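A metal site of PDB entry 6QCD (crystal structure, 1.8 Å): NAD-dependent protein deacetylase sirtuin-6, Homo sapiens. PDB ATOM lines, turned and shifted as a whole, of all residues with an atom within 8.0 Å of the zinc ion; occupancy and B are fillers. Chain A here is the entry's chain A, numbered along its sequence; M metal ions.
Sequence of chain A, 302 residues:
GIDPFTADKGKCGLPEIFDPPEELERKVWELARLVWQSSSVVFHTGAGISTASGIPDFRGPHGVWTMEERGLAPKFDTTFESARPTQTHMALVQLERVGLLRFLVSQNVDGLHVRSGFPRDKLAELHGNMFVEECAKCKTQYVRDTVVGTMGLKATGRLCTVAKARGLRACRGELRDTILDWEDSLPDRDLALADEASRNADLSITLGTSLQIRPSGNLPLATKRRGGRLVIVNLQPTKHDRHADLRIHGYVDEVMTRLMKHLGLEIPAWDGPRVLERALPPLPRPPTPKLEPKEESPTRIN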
ATOM      1  N   GLU A 134      -2.030  25.917 -27.769  1.00  0.00           N
ATOM      2  CA  GLU A 134      -2.495  25.272 -26.535  1.00  0.00           C
ATOM      3  C   GLU A 134      -2.674  26.337 -25.427  1.00  0.00           C
ATOM      4  O   GLU A 134      -1.730  27.142 -25.259  1.00  0.00           O
ATOM      5  CB  GLU A 134      -1.451  24.252 -26.109  1.00  0.00           C
ATOM      6  CG  GLU A 134      -1.853  23.467 -24.861  1.00  0.00           C
ATOM      7  CD  GLU A 134      -0.853  22.380 -24.580  1.00  0.00           C
ATOM      8  OE1 GLU A 134      -0.857  21.374 -25.326  1.00  0.00           O
ATOM      9  OE2 GLU A 134       0.025  22.614 -23.714  1.00  0.00           O
ATOM     10  N   CYS A 135      -3.780  26.293 -24.675  1.00  0.00           N
ATOM     11  CA  CYS A 135      -4.007  27.228 -23.529  1.00  0.00           C
ATOM     12  C   CYS A 135      -3.027  26.840 -22.404  1.00  0.00           C
ATOM     13  O   CYS A 135      -3.108  25.657 -21.900  1.00  0.00           O
ATOM     14  CB  CYS A 135      -5.438  27.214 -23.007  1.00  0.00           C
ATOM     15  SG  CYS A 135      -5.724  28.285 -21.560  1.00  0.00           S
ATOM     16  N   ALA A 136      -2.138  27.760 -22.062  1.00  0.00           N
ATOM     17  CA  ALA A 136      -1.215  27.620 -20.910  1.00  0.00           C
ATOM     18  C   ALA A 136      -2.005  27.365 -19.605  1.00  0.00           C
ATOM     19  O   ALA A 136      -1.498  26.571 -18.758  1.00  0.00           O
ATOM     20  CB  ALA A 136      -0.292  28.818 -20.812  1.00  0.00           C
ATOM     21  N   LYS A 137      -3.226  27.893 -19.456  1.00  0.00           N
ATOM     22  CA  LYS A 137      -4.082  27.626 -18.264  1.00  0.00           C
ATOM     23  C   LYS A 137      -4.726  26.242 -18.363  1.00  0.00           C
ATOM     24  O   LYS A 137      -4.345  25.386 -17.534  1.00  0.00           O
ATOM     25  CB  LYS A 137      -5.175  28.683 -18.030  1.00  0.00           C
ATOM     26  CG  LYS A 137      -4.625  30.091 -17.771  1.00  0.00           C
ATOM     27  CD  LYS A 137      -5.592  31.080 -17.146  1.00  0.00           C
ATOM     28  CE  LYS A 137      -4.902  32.335 -16.645  1.00  0.00           C
ATOM     29  NZ  LYS A 137      -5.641  33.575 -17.006  1.00  0.00           N
ATOM     30  N   CYS A 138      -5.712  26.035 -19.242  1.00  0.00           N
ATOM     31  CA  CYS A 138      -6.601  24.843 -19.197  1.00  0.00           C
ATOM     32  C   CYS A 138      -6.090  23.712 -20.112  1.00  0.00           C
ATOM     33  O   CYS A 138      -6.677  22.643 -20.052  1.00  0.00           O
ATOM     34  CB  CYS A 138      -8.054  25.218 -19.508  1.00  0.00           C
ATOM     35  SG  CYS A 138      -8.353  25.788 -21.206  1.00  0.00           S
ATOM     36  N   LYS A 139      -5.065  23.954 -20.937  1.00  0.00           N
ATOM     37  CA  LYS A 139      -4.408  22.952 -21.831  1.00  0.00           C
ATOM     38  C   LYS A 139      -5.245  22.642 -23.059  1.00  0.00           C
ATOM     39  O   LYS A 139      -4.843  21.734 -23.838  1.00  0.00           O
ATOM     40  CB  LYS A 139      -4.179  21.603 -21.132  1.00  0.00           C
ATOM     41  CG  LYS A 139      -3.346  21.655 -19.881  1.00  0.00           C
ATOM     42  CD  LYS A 139      -1.979  22.261 -20.077  1.00  0.00           C
ATOM     43  CE  LYS A 139      -1.121  22.125 -18.831  1.00  0.00           C
ATOM     44  NZ  LYS A 139      -0.307  23.347 -18.614  1.00  0.00           N
ATOM     45  N   THR A 140      -6.390  23.298 -23.234  1.00  0.00           N
ATOM     46  CA  THR A 140      -7.198  23.149 -24.463  1.00  0.00           C
ATOM     47  C   THR A 140      -6.309  23.491 -25.662  1.00  0.00           C
ATOM     48  O   THR A 140      -5.657  24.544 -25.635  1.00  0.00           O
ATOM     49  CB  THR A 140      -8.448  24.032 -24.461  1.00  0.00           C
ATOM     50  OG1 THR A 140      -9.332  23.607 -23.409  1.00  0.00           O
ATOM     51  CG2 THR A 140      -9.193  23.973 -25.776  1.00  0.00           C
ATOM     52  N   GLN A 141      -6.412  22.689 -26.715  1.00  0.00           N
ATOM     53  CA  GLN A 141      -5.644  22.824 -27.970  1.00  0.00           C
ATOM     54  C   GLN A 141      -6.585  23.333 -29.063  1.00  0.00           C
ATOM     55  O   GLN A 141      -7.752  22.959 -29.093  1.00  0.00           O
ATOM     56  CB  GLN A 141      -5.030  21.476 -28.338  1.00  0.00           C
ATOM     57  CG  GLN A 141      -3.856  21.160 -27.429  1.00  0.00           C
ATOM     58  CD  GLN A 141      -3.092  19.929 -27.829  1.00  0.00           C
ATOM     59  OE1 GLN A 141      -3.563  19.126 -28.628  1.00  0.00           O
ATOM     60  NE2 GLN A 141      -1.875  19.831 -27.328  1.00  0.00           N
ATOM     61  N   TYR A 142      -6.081  24.230 -29.865  1.00  0.00           N
ATOM     62  CA  TYR A 142      -6.790  24.822 -31.009  1.00  0.00           C
ATOM     63  C   TYR A 142      -6.063  24.389 -32.288  1.00  0.00           C
ATOM     64  O   TYR A 142      -4.848  24.639 -32.363  1.00  0.00           O
ATOM     65  CB  TYR A 142      -6.772  26.330 -30.831  1.00  0.00           C
ATOM     66  CG  TYR A 142      -7.532  26.774 -29.610  1.00  0.00           C
ATOM     67  CD1 TYR A 142      -6.952  26.788 -28.350  1.00  0.00           C
ATOM     68  CD2 TYR A 142      -8.861  27.158 -29.719  1.00  0.00           C
ATOM     69  CE1 TYR A 142      -7.670  27.195 -27.239  1.00  0.00           C
ATOM     70  CE2 TYR A 142      -9.594  27.551 -28.621  1.00  0.00           C
ATOM     71  CZ  TYR A 142      -8.995  27.561 -27.372  1.00  0.00           C
ATOM     72  OH  TYR A 142      -9.741  27.950 -26.284  1.00  0.00           O
ATOM     73  N   LEU A 159      -5.874  34.350 -27.102  1.00  0.00           N
ATOM     74  CA  LEU A 159      -6.383  33.978 -25.765  1.00  0.00           C
ATOM     75  C   LEU A 159      -7.383  32.842 -25.891  1.00  0.00           C
ATOM     76  O   LEU A 159      -8.093  32.780 -26.892  1.00  0.00           O
ATOM     77  CB  LEU A 159      -7.058  35.185 -25.096  1.00  0.00           C
ATOM     78  CG  LEU A 159      -6.116  36.252 -24.535  1.00  0.00           C
ATOM     79  CD1 LEU A 159      -6.907  37.241 -23.690  1.00  0.00           C
ATOM     80  CD2 LEU A 159      -4.999  35.640 -23.720  1.00  0.00           C
ATOM     81  N   CYS A 160      -7.498  32.022 -24.850  1.00  0.00           N
ATOM     82  CA  CYS A 160      -8.419  30.892 -24.793  1.00  0.00           C
ATOM     83  C   CYS A 160      -9.890  31.345 -24.733  1.00  0.00           C
ATOM     84  O   CYS A 160     -10.192  32.336 -24.063  1.00  0.00           O
ATOM     85  CB  CYS A 160      -8.023  30.050 -23.596  1.00  0.00           C
ATOM     86  SG  CYS A 160      -8.964  28.528 -23.459  1.00  0.00           S
ATOM     87  N   THR A 161     -10.787  30.624 -25.405  1.00  0.00           N
ATOM     88  CA  THR A 161     -12.210  30.979 -25.537  1.00  0.00           C
ATOM     89  C   THR A 161     -13.104  29.942 -24.854  1.00  0.00           C
ATOM     90  O   THR A 161     -14.308  30.114 -24.955  1.00  0.00           O
ATOM     91  CB  THR A 161     -12.537  31.199 -27.015  1.00  0.00           C
ATOM     92  OG1 THR A 161     -12.356  29.967 -27.727  1.00  0.00           O
ATOM     93  CG2 THR A 161     -11.703  32.268 -27.650  1.00  0.00           C
ATOM     94  N   VAL A 162     -12.584  28.876 -24.241  1.00  0.00           N
ATOM     95  CA  VAL A 162     -13.420  27.929 -23.450  1.00  0.00           C
ATOM     96  C   VAL A 162     -14.344  28.732 -22.514  1.00  0.00           C
ATOM     97  O   VAL A 162     -13.894  29.784 -21.994  1.00  0.00           O
ATOM     98  CB  VAL A 162     -12.565  26.916 -22.662  1.00  0.00           C
ATOM     99  CG1 VAL A 162     -13.439  25.894 -21.925  1.00  0.00           C
ATOM    100  CG2 VAL A 162     -11.584  26.181 -23.546  1.00  0.00           C
ATOM    101  N   ALA A 163     -15.581  28.242 -22.310  1.00  0.00           N
ATOM    102  CA  ALA A 163     -16.752  28.954 -21.732  1.00  0.00           C
ATOM    103  C   ALA A 163     -16.390  29.598 -20.380  1.00  0.00           C
ATOM    104  O   ALA A 163     -16.068  28.829 -19.452  1.00  0.00           O
ATOM    105  CB  ALA A 163     -17.918  27.995 -21.596  1.00  0.00           C
ATOM    106  N   CYS A 171     -12.141  31.488 -19.960  1.00  0.00           N
ATOM    107  CA  CYS A 171     -10.771  31.114 -19.504  1.00  0.00           C
ATOM    108  C   CYS A 171      -9.800  32.274 -19.699  1.00  0.00           C
ATOM    109  O   CYS A 171      -9.083  32.609 -18.749  1.00  0.00           O
ATOM    110  CB  CYS A 171     -10.267  29.877 -20.235  1.00  0.00           C
ATOM    111  SG  CYS A 171      -8.554  29.458 -19.786  1.00  0.00           S
ATOM    112  N   ARG A 172      -9.757  32.838 -20.908  1.00  0.00           N
ATOM    113  CA  ARG A 172      -8.830  33.916 -21.341  1.00  0.00           C
ATOM    114  C   ARG A 172      -7.368  33.514 -21.075  1.00  0.00           C
ATOM    115  O   ARG A 172      -6.512  34.394 -21.106  1.00  0.00           O
ATOM    116  CB  ARG A 172      -9.217  35.244 -20.677  1.00  0.00           C
ATOM    117  CG  ARG A 172     -10.710  35.526 -20.751  1.00  0.00           C
ATOM    118  CD  ARG A 172     -11.094  36.901 -20.231  1.00  0.00           C
ATOM    119  NE  ARG A 172     -10.337  37.941 -20.921  1.00  0.00           N
ATOM    120  CZ  ARG A 172     -10.545  38.348 -22.173  1.00  0.00           C
ATOM    121  NH1 ARG A 172     -11.507  37.807 -22.901  1.00  0.00           N
ATOM    122  NH2 ARG A 172      -9.799  39.307 -22.685  1.00  0.00           N
ATOM    123  N   GLY A 173      -7.091  32.220 -20.896  1.00  0.00           N
ATOM    124  CA  GLY A 173      -5.710  31.707 -20.812  1.00  0.00           C
ATOM    125  C   GLY A 173      -4.899  32.111 -22.039  1.00  0.00           C
ATOM    126  O   GLY A 173      -5.486  32.302 -23.128  1.00  0.00           O
ATOM    127  N   GLU A 174      -3.588  32.260 -21.840  1.00  0.00           N
ATOM    128  CA  GLU A 174      -2.601  32.639 -22.883  1.00  0.00           C
ATOM    129  C   GLU A 174      -2.397  31.440 -23.823  1.00  0.00           C
ATOM    130  O   GLU A 174      -2.142  30.329 -23.313  1.00  0.00           O
ATOM    131  CB  GLU A 174      -1.294  33.023 -22.202  1.00  0.00           C
ATOM    132  CG  GLU A 174      -0.218  33.494 -23.149  1.00  0.00           C
ATOM    133  CD  GLU A 174       1.066  33.853 -22.402  1.00  0.00           C
ATOM    134  OE1 GLU A 174       1.786  32.902 -21.955  1.00  0.00           O
ATOM    135  OE2 GLU A 174       1.319  35.073 -22.232  1.00  0.00           O
ATOM    136  N   LEU A 175      -2.540  31.634 -25.136  1.00  0.00           N
ATOM    137  CA  LEU A 175      -2.247  30.565 -26.126  1.00  0.00           C
ATOM    138  C   LEU A 175      -0.754  30.557 -26.449  1.00  0.00           C
ATOM    139  O   LEU A 175      -0.190  31.629 -26.671  1.00  0.00           O
ATOM    140  CB  LEU A 175      -3.087  30.761 -27.381  1.00  0.00           C
ATOM    141  CG  LEU A 175      -4.593  30.685 -27.154  1.00  0.00           C
ATOM    142  CD1 LEU A 175      -5.329  30.624 -28.470  1.00  0.00           C
ATOM    143  CD2 LEU A 175      -4.983  29.550 -26.237  1.00  0.00           C
HETATM  144 ZN    ZN M   1      -7.930  27.917 -21.482  1.00  0.00          ZN
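Of the 19 residues printed, 4 come within 4 Å of the zinc ion.
The zinc ion is bound by SG of Cys 138 (2.2 Å), SG of Cys 135 (2.2 Å), SG of Cys 160 (2.3 Å) and SG of Cys 171 (2.4 Å).
N of Cys 160 lies within hydrogen-bond range of O of Gly 173.
N of Gly 173 sits close to SG of Cys 171, at 3.3 Å.
N of Arg 172 is in hydrogen-bond range of O of Cys 160, 3.2 Å away.
The side-chain sulfur (SG) of Cys 160 lies close to the side-chain hydroxyl (OH) of Tyr 142 (3.0 Å).
N of Cys 171 is in hydrogen-bond range of O of Val 162.
The side-chain hydroxyl of Thr 140 lies close to the side-chain sulfur of Cys 138 (3.3 Å).
The side-chain sulfur (SG) of Cys 135 lies close to the backbone NH (N) of Lys 137, at 3.3 Å.
The backbone NH (N) of Cys 135 sits at hydrogen-bond distance from the backbone carbonyl oxygen (O) of Thr 140.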
